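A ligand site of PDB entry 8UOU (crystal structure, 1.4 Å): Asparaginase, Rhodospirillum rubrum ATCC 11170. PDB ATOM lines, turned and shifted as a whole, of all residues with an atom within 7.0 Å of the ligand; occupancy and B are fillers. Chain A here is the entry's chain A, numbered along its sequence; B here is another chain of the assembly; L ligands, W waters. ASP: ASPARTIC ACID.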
ATOM      1  N   GLY A  27      19.706   4.704   5.082  1.00  0.00           N
ATOM      2  CA  GLY A  27      19.326   3.286   5.081  1.00  0.00           C
ATOM      3  C   GLY A  27      19.501   2.618   3.725  1.00  0.00           C
ATOM      4  O   GLY A  27      20.469   2.920   3.012  1.00  0.00           O
ATOM      5  N   GLY A  28      18.636   1.669   3.407  1.00  0.00           N
ATOM      6  CA  GLY A  28      18.687   0.916   2.162  1.00  0.00           C
ATOM      7  C   GLY A  28      19.275  -0.483   2.331  1.00  0.00           C
ATOM      8  O   GLY A  28      19.805  -0.841   3.407  1.00  0.00           O
ATOM      9  N   THR A  29      19.200  -1.224   1.241  1.00  0.00           N
ATOM     10  CA  THR A  29      19.766  -2.580   1.184  1.00  0.00           C
ATOM     11  C   THR A  29      21.241  -2.568   1.649  1.00  0.00           C
ATOM     12  O   THR A  29      21.632  -3.506   2.323  1.00  0.00           O
ATOM     13  CB  THR A  29      19.614  -3.188  -0.204  1.00  0.00           C
ATOM     14  OG1 THR A  29      18.217  -3.459  -0.381  1.00  0.00           O
ATOM     15  CG2 THR A  29      20.353  -4.451  -0.444  1.00  0.00           C
ATOM     16  N   ILE A  30      22.007  -1.531   1.296  1.00  0.00           N
ATOM     17  CA  ILE A  30      23.423  -1.475   1.679  1.00  0.00           C
ATOM     18  C   ILE A  30      23.584  -1.792   3.162  1.00  0.00           C
ATOM     19  O   ILE A  30      24.591  -2.426   3.547  1.00  0.00           O
ATOM     20  CB  ILE A  30      24.011  -0.110   1.276  1.00  0.00           C
ATOM     21  CG1 ILE A  30      25.512  -0.102   1.588  1.00  0.00           C
ATOM     22  CG2 ILE A  30      23.337   1.122   1.845  1.00  0.00           C
ATOM     23  CD1 ILE A  30      26.298   1.041   0.890  1.00  0.00           C
ATOM     24  N   LYS A  32      21.471  -3.438   5.297  1.00  0.00           N
ATOM     25  CA  LYS A  32      20.656  -4.526   5.895  1.00  0.00           C
ATOM     26  C   LYS A  32      21.527  -5.515   6.666  1.00  0.00           C
ATOM     27  O   LYS A  32      22.701  -5.805   6.252  1.00  0.00           O
ATOM     28  CB  LYS A  32      19.833  -5.201   4.804  1.00  0.00           C
ATOM     29  CG  LYS A  32      18.599  -4.380   4.413  1.00  0.00           C
ATOM     30  CD  LYS A  32      17.831  -4.982   3.298  1.00  0.00           C
ATOM     31  CE  LYS A  32      16.683  -4.051   2.896  1.00  0.00           C
ATOM     32  NZ  LYS A  32      15.816  -4.662   1.845  1.00  0.00           N
ATOM     33  N   VAL A  43      17.083  -3.044   8.360  1.00  0.00           N
ATOM     34  CA  VAL A  43      18.060  -1.999   8.004  1.00  0.00           C
ATOM     35  C   VAL A  43      18.801  -1.708   9.305  1.00  0.00           C
ATOM     36  O   VAL A  43      18.221  -1.267  10.301  1.00  0.00           O
ATOM     37  CB  VAL A  43      17.369  -0.791   7.377  1.00  0.00           C
ATOM     38  CG1 VAL A  43      18.380   0.280   7.106  1.00  0.00           C
ATOM     39  CG2 VAL A  43      16.593  -1.166   6.105  1.00  0.00           C
ATOM     40  N   LYS A  69      15.796   3.382   7.014  1.00  0.00           N
ATOM     41  CA  LYS A  69      14.600   2.838   6.311  1.00  0.00           C
ATOM     42  C   LYS A  69      14.974   2.146   5.000  1.00  0.00           C
ATOM     43  O   LYS A  69      15.986   2.481   4.368  1.00  0.00           O
ATOM     44  CB  LYS A  69      13.618   3.961   5.991  1.00  0.00           C
ATOM     45  CG  LYS A  69      12.891   4.511   7.209  1.00  0.00           C
ATOM     46  CD  LYS A  69      11.708   5.374   6.797  1.00  0.00           C
ATOM     47  CE  LYS A  69      11.129   6.210   7.890  1.00  0.00           C
ATOM     48  NZ  LYS A  69       9.847   6.817   7.433  1.00  0.00           N
ATOM     49  N   ASP A  70      14.176   1.177   4.599  1.00  0.00           N
ATOM     50  CA  ASP A  70      14.073   0.706   3.203  1.00  0.00           C
ATOM     51  C   ASP A  70      13.519   1.910   2.462  1.00  0.00           C
ATOM     52  O   ASP A  70      12.519   2.512   2.958  1.00  0.00           O
ATOM     53  CB  ASP A  70      13.230  -0.577   3.100  1.00  0.00           C
ATOM     54  CG  ASP A  70      13.233  -1.265   1.773  1.00  0.00           C
ATOM     55  OD1 ASP A  70      13.029  -0.564   0.767  1.00  0.00           O
ATOM     56  OD2 ASP A  70      13.515  -2.534   1.725  1.00  0.00           O
ATOM     57  N   SER A  71      14.100   2.259   1.319  1.00  0.00           N
ATOM     58  CA  SER A  71      13.666   3.463   0.593  1.00  0.00           C
ATOM     59  C   SER A  71      12.239   3.293   0.054  1.00  0.00           C
ATOM     60  O   SER A  71      11.641   4.322  -0.278  1.00  0.00           O
ATOM     61  CB  SER A  71      14.623   3.869  -0.496  1.00  0.00           C
ATOM     62  OG  SER A  71      14.556   3.132  -1.698  1.00  0.00           O
ATOM     63  N   LEU A  72      11.720   2.073  -0.063  1.00  0.00           N
ATOM     64  CA  LEU A  72      10.275   1.870  -0.411  1.00  0.00           C
ATOM     65  C   LEU A  72       9.394   2.588   0.598  1.00  0.00           C
ATOM     66  O   LEU A  72       8.282   2.980   0.273  1.00  0.00           O
ATOM     67  CB  LEU A  72       9.981   0.378  -0.394  1.00  0.00           C
ATOM     68  CG  LEU A  72      10.635  -0.384  -1.557  1.00  0.00           C
ATOM     69  CD1 LEU A  72      10.434  -1.874  -1.426  1.00  0.00           C
ATOM     70  CD2 LEU A  72      10.078   0.097  -2.874  1.00  0.00           C
ATOM     71  N   ASP A  73       9.854   2.758   1.836  1.00  0.00           N
ATOM     72  CA  ASP A  73       9.085   3.314   2.966  1.00  0.00           C
ATOM     73  C   ASP A  73       9.212   4.824   3.016  1.00  0.00           C
ATOM     74  O   ASP A  73       8.638   5.385   3.914  1.00  0.00           O
ATOM     75  CB  ASP A  73       9.403   2.572   4.259  1.00  0.00           C
ATOM     76  CG  ASP A  73       8.909   1.131   4.142  1.00  0.00           C
ATOM     77  OD1 ASP A  73       7.740   0.905   3.658  1.00  0.00           O
ATOM     78  OD2 ASP A  73       9.638   0.228   4.575  1.00  0.00           O
ATOM     79  N   HIS A  98      21.750   5.359   0.652  1.00  0.00           N
ATOM     80  CA  HIS A  98      20.261   5.320   0.540  1.00  0.00           C
ATOM     81  C   HIS A  98      19.875   4.016  -0.160  1.00  0.00           C
ATOM     82  O   HIS A  98      20.641   3.449  -0.923  1.00  0.00           O
ATOM     83  CB  HIS A  98      19.864   6.626  -0.223  1.00  0.00           C
ATOM     84  CG  HIS A  98      18.435   7.028  -0.372  1.00  0.00           C
ATOM     85  ND1 HIS A  98      17.560   6.368  -1.170  1.00  0.00           N
ATOM     86  CD2 HIS A  98      17.853   8.225  -0.088  1.00  0.00           C
ATOM     87  CE1 HIS A  98      16.373   7.039  -1.156  1.00  0.00           C
ATOM     88  NE2 HIS A  98      16.528   8.200  -0.512  1.00  0.00           N
ATOM     89  N   GLY A  99      18.600   3.644   0.042  1.00  0.00           N
ATOM     90  CA  GLY A  99      18.037   2.581  -0.779  1.00  0.00           C
ATOM     91  C   GLY A  99      17.958   2.918  -2.232  1.00  0.00           C
ATOM     92  O   GLY A  99      17.789   4.062  -2.594  1.00  0.00           O
ATOM     93  N   THR A 100      18.081   1.940  -3.139  1.00  0.00           N
ATOM     94  CA  THR A 100      18.106   2.171  -4.594  1.00  0.00           C
ATOM     95  C   THR A 100      16.679   2.312  -5.152  1.00  0.00           C
ATOM     96  O   THR A 100      16.562   2.838  -6.216  1.00  0.00           O
ATOM     97  CB  THR A 100      18.897   1.104  -5.342  1.00  0.00           C
ATOM     98  OG1 THR A 100      18.289  -0.185  -5.235  1.00  0.00           O
ATOM     99  CG2 THR A 100      20.328   1.048  -4.865  1.00  0.00           C
ATOM    100  N   ASP A 101      15.662   1.756  -4.497  1.00  0.00           N
ATOM    101  CA  ASP A 101      14.313   1.704  -5.083  1.00  0.00           C
ATOM    102  C   ASP A 101      13.703   3.096  -5.269  1.00  0.00           C
ATOM    103  O   ASP A 101      13.001   3.272  -6.310  1.00  0.00           O
ATOM    104  CB  ASP A 101      13.399   0.729  -4.344  1.00  0.00           C
ATOM    105  CG  ASP A 101      13.650  -0.716  -4.762  1.00  0.00           C
ATOM    106  OD1 ASP A 101      14.260  -0.961  -5.902  1.00  0.00           O
ATOM    107  OD2 ASP A 101      13.398  -1.590  -3.884  1.00  0.00           O
ATOM    108  N   THR A 102      13.918   4.013  -4.331  1.00  0.00           N
ATOM    109  CA  THR A 102      13.448   5.391  -4.530  1.00  0.00           C
ATOM    110  C   THR A 102      14.524   6.429  -4.450  1.00  0.00           C
ATOM    111  O   THR A 102      14.281   7.622  -4.226  1.00  0.00           O
ATOM    112  CB  THR A 102      12.258   5.729  -3.598  1.00  0.00           C
ATOM    113  OG1 THR A 102      12.731   5.903  -2.253  1.00  0.00           O
ATOM    114  CG2 THR A 102      11.133   4.703  -3.682  1.00  0.00           C
ATOM    115  N   MET A 103      15.710   5.980  -4.750  1.00  0.00           N
ATOM    116  CA  MET A 103      16.874   6.889  -4.847  1.00  0.00           C
ATOM    117  C   MET A 103      16.647   7.988  -5.899  1.00  0.00           C
ATOM    118  O   MET A 103      17.023   9.155  -5.675  1.00  0.00           O
ATOM    119  CB  MET A 103      18.059   6.022  -5.223  1.00  0.00           C
ATOM    120  CG  MET A 103      19.414   6.746  -5.170  1.00  0.00           C
ATOM    121  SD  MET A 103      20.887   5.809  -5.442  1.00  0.00           S
ATOM    122  CE  MET A 103      21.031   4.949  -3.900  1.00  0.00           C
ATOM    123  N   GLY A 125      24.424   3.529  -2.872  1.00  0.00           N
ATOM    124  CA  GLY A 125      24.005   2.431  -2.027  1.00  0.00           C
ATOM    125  C   GLY A 125      24.495   1.154  -2.599  1.00  0.00           C
ATOM    126  O   GLY A 125      25.636   1.124  -3.096  1.00  0.00           O
ATOM    127  N   ALA A 126      23.771   0.068  -2.446  1.00  0.00           N
ATOM    128  CA  ALA A 126      24.181  -1.252  -2.928  1.00  0.00           C
ATOM    129  C   ALA A 126      22.992  -2.104  -3.218  1.00  0.00           C
ATOM    130  O   ALA A 126      21.998  -2.077  -2.464  1.00  0.00           O
ATOM    131  CB  ALA A 126      25.130  -1.902  -1.908  1.00  0.00           C
ATOM    132  N   MET A 127      23.066  -2.865  -4.285  1.00  0.00           N
ATOM    133  CA  MET A 127      21.991  -3.799  -4.621  1.00  0.00           C
ATOM    134  C   MET A 127      21.987  -5.016  -3.690  1.00  0.00           C
ATOM    135  O   MET A 127      20.979  -5.687  -3.631  1.00  0.00           O
ATOM    136  CB  MET A 127      22.090  -4.219  -6.095  1.00  0.00           C
ATOM    137  CG  MET A 127      22.089  -3.051  -7.135  1.00  0.00           C
ATOM    138  SD  MET A 127      20.591  -2.144  -7.002  1.00  0.00           S
ATOM    139  CE  MET A 127      20.822  -0.876  -8.253  1.00  0.00           C
ATOM    140  N   VAL A 128      23.140  -5.344  -3.121  1.00  0.00           N
ATOM    141  CA  VAL A 128      23.322  -6.484  -2.191  1.00  0.00           C
ATOM    142  C   VAL A 128      23.830  -5.921  -0.879  1.00  0.00           C
ATOM    143  O   VAL A 128      24.722  -5.068  -0.892  1.00  0.00           O
ATOM    144  CB  VAL A 128      24.321  -7.509  -2.771  1.00  0.00           C
ATOM    145  CG1 VAL A 128      24.629  -8.590  -1.742  1.00  0.00           C
ATOM    146  CG2 VAL A 128      23.820  -8.099  -4.093  1.00  0.00           C
ATOM    147  N   MET A 159      26.469   4.687  -9.327  1.00  0.00           N
ATOM    148  CA  MET A 159      26.201   3.252  -9.229  1.00  0.00           C
ATOM    149  C   MET A 159      26.759   2.590 -10.497  1.00  0.00           C
ATOM    150  O   MET A 159      26.854   3.267 -11.541  1.00  0.00           O
ATOM    151  CB  MET A 159      24.693   3.008  -9.094  1.00  0.00           C
ATOM    152  CG  MET A 159      24.100   3.426  -7.736  1.00  0.00           C
ATOM    153  SD  MET A 159      24.716   2.466  -6.327  1.00  0.00           S
ATOM    154  CE  MET A 159      23.968   0.868  -6.580  1.00  0.00           C
ATOM    155  N   LYS A 171      15.204   3.457 -12.074  1.00  0.00           N
ATOM    156  CA  LYS A 171      15.514   2.118 -11.544  1.00  0.00           C
ATOM    157  C   LYS A 171      14.751   1.043 -12.294  1.00  0.00           C
ATOM    158  O   LYS A 171      13.502   1.110 -12.312  1.00  0.00           O
ATOM    159  CB  LYS A 171      15.251   2.045 -10.038  1.00  0.00           C
ATOM    160  CG  LYS A 171      15.572   0.691  -9.392  1.00  0.00           C
ATOM    161  CD  LYS A 171      16.993   0.312  -9.242  1.00  0.00           C
ATOM    162  CE  LYS A 171      17.133  -1.130  -8.766  1.00  0.00           C
ATOM    163  NZ  LYS A 171      16.708  -1.354  -7.348  1.00  0.00           N
ATOM    164  N   TYR B  34      20.650 -13.379  -0.193  1.00  0.00           N
ATOM    165  CA  TYR B  34      19.876 -12.241  -0.696  1.00  0.00           C
ATOM    166  C   TYR B  34      19.490 -12.425  -2.151  1.00  0.00           C
ATOM    167  O   TYR B  34      20.224 -12.856  -3.006  1.00  0.00           O
ATOM    168  CB  TYR B  34      20.681 -10.944  -0.542  1.00  0.00           C
ATOM    169  CG  TYR B  34      19.822  -9.713  -0.654  1.00  0.00           C
ATOM    170  CD1 TYR B  34      19.125  -9.263   0.443  1.00  0.00           C
ATOM    171  CD2 TYR B  34      19.768  -8.968  -1.809  1.00  0.00           C
ATOM    172  CE1 TYR B  34      18.309  -8.148   0.370  1.00  0.00           C
ATOM    173  CE2 TYR B  34      18.962  -7.845  -1.886  1.00  0.00           C
ATOM    174  CZ  TYR B  34      18.243  -7.429  -0.795  1.00  0.00           C
ATOM    175  OH  TYR B  34      17.457  -6.301  -0.908  1.00  0.00           O
ATOM    176  N   LEU B  36      17.653  -9.950  -5.086  1.00  0.00           N
ATOM    177  CA  LEU B  36      17.169  -8.588  -5.419  1.00  0.00           C
ATOM    178  C   LEU B  36      15.674  -8.634  -5.791  1.00  0.00           C
ATOM    179  O   LEU B  36      14.964  -7.724  -5.405  1.00  0.00           O
ATOM    180  CB  LEU B  36      17.931  -8.059  -6.652  1.00  0.00           C
ATOM    181  CG  LEU B  36      19.239  -7.342  -6.451  1.00  0.00           C
ATOM    182  CD1 LEU B  36      20.280  -8.259  -5.886  1.00  0.00           C
ATOM    183  CD2 LEU B  36      19.737  -6.817  -7.800  1.00  0.00           C
ATOM    184  N   ASN B  39      13.703  -8.518  -2.732  1.00  0.00           N
ATOM    185  CA  ASN B  39      14.019  -7.467  -1.728  1.00  0.00           C
ATOM    186  C   ASN B  39      14.243  -8.134  -0.354  1.00  0.00           C
ATOM    187  O   ASN B  39      13.814  -7.561   0.663  1.00  0.00           O
ATOM    188  CB  ASN B  39      12.922  -6.392  -1.659  1.00  0.00           C
ATOM    189  CG  ASN B  39      13.295  -5.171  -0.855  1.00  0.00           C
ATOM    190  OD1 ASN B  39      14.455  -4.776  -0.896  1.00  0.00           O
ATOM    191  ND2 ASN B  39      12.420  -4.599  -0.045  1.00  0.00           N
HETATM  192  N   ASP L   1      14.374  -1.935  -1.235  1.00  0.00           N
HETATM  193  CA  ASP L   1      15.790  -1.524  -1.088  1.00  0.00           C
HETATM  194  C   ASP L   1      15.739  -0.038  -0.798  1.00  0.00           C
HETATM  195  O   ASP L   1      15.450   0.721  -1.760  1.00  0.00           O
HETATM  196  CB  ASP L   1      16.581  -1.856  -2.375  1.00  0.00           C
HETATM  197  CG  ASP L   1      18.043  -1.423  -2.439  1.00  0.00           C
HETATM  198  OD1 ASP L   1      18.463  -0.543  -1.605  1.00  0.00           O
HETATM  199  OD2 ASP L   1      18.727  -1.968  -3.360  1.00  0.00           O
HETATM  200  OXT ASP L   1      15.981   0.344   0.345  1.00  0.00           O
HETATM  201  O   HOH W   1      21.129   0.536  -0.957  1.00  0.00           O
HETATM  202  O   HOH W   2      18.603  -4.451  -4.346  1.00  0.00           O
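An oxygen (OD2) of the ligand lies close to the backbone carbonyl oxygen (O) of Ala 126 (3.4 Å).
Residues that only touch the ligand: Gly 99, Gly 28, Leu 72 and Met 127.
Hydrophobic or aromatic side chains that line the ligand: Leu 72.
11 residues have an atom within 4 Å of the ligand: Gly 28, Thr 29, Asp 70, Ser 71, Leu 72, Gly 99, Thr 100, Asp 101, Ala 126, Met 127 and Asn 39 of chain B.
The nearest printed residue that does not touch the ligand is Lys 32 (4.3 Å).
The backbone NH (N) of Ser 71 sits at hydrogen-bond distance from an oxygen (OXT) of the ligand (2.9 Å).
The side-chain hydroxyl of Ser 71 lies within hydrogen-bond range of an oxygen (O) of the ligand (2.6 Å).
An oxygen (OD1) of the ligand is in hydrogen-bond range of the backbone NH (N) of Thr 100 (2.9 Å).
OD2 of the ligand is in hydrogen-bond range of OG1 of Thr 100, at 2.6 Å.
A nitrogen (N) of the ligand is in salt-bridge range of the side-chain carboxylate (OD1) of Asp 70, 2.8 Å away.
The backbone NH (N) of Asp 101 lies within hydrogen-bond range of an oxygen (O) of the ligand, at 2.9 Å.
OD2 of Asp 101 lies within salt-bridge range of N of the ligand, 2.8 Å away.
A nitrogen (N) of the ligand is in hydrogen-bond range of the side-chain amide oxygen (OD1) of Asn 39 of chain B (2.9 Å).
N of Thr 29 sits at hydrogen-bond distance from OD1 of the ligand (3.0 Å).
An oxygen (OD1) of the ligand sits close to the side-chain hydroxyl (OG1) of Thr 29, 3.2 Å away.
OG of Ser 71 sits close to O of Gly 99.
The side-chain hydroxyl (OG1) of Thr 100 sits at hydrogen-bond distance from the side-chain sulfur (SD) of Met 127 (3.5 Å).
OG1 of Thr 100 is in hydrogen-bond range of NZ of Lys 171.
OD1 of Asp 70 sits at hydrogen-bond distance from N of Leu 72.
The side-chain carboxylate of Asp 70 lies within salt-bridge range of the side-chain amino group of Lys 32.
The side-chain carboxylate (OD1) of Asp 101 is in salt-bridge range of the side-chain amino group (NZ) of Lys 171 (2.9 Å).
OD1 of Asn 39 of chain B sits at hydrogen-bond distance from NZ of Lys 32, at 3.1 Å.
The backbone NH (N) of Gly 28 is in hydrogen-bond range of the backbone carbonyl oxygen (O) of Lys 69 (2.9 Å).
Water W2 bridges OD2 of the ligand (2.7 Å) and O of Met 127 (2.8 Å).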
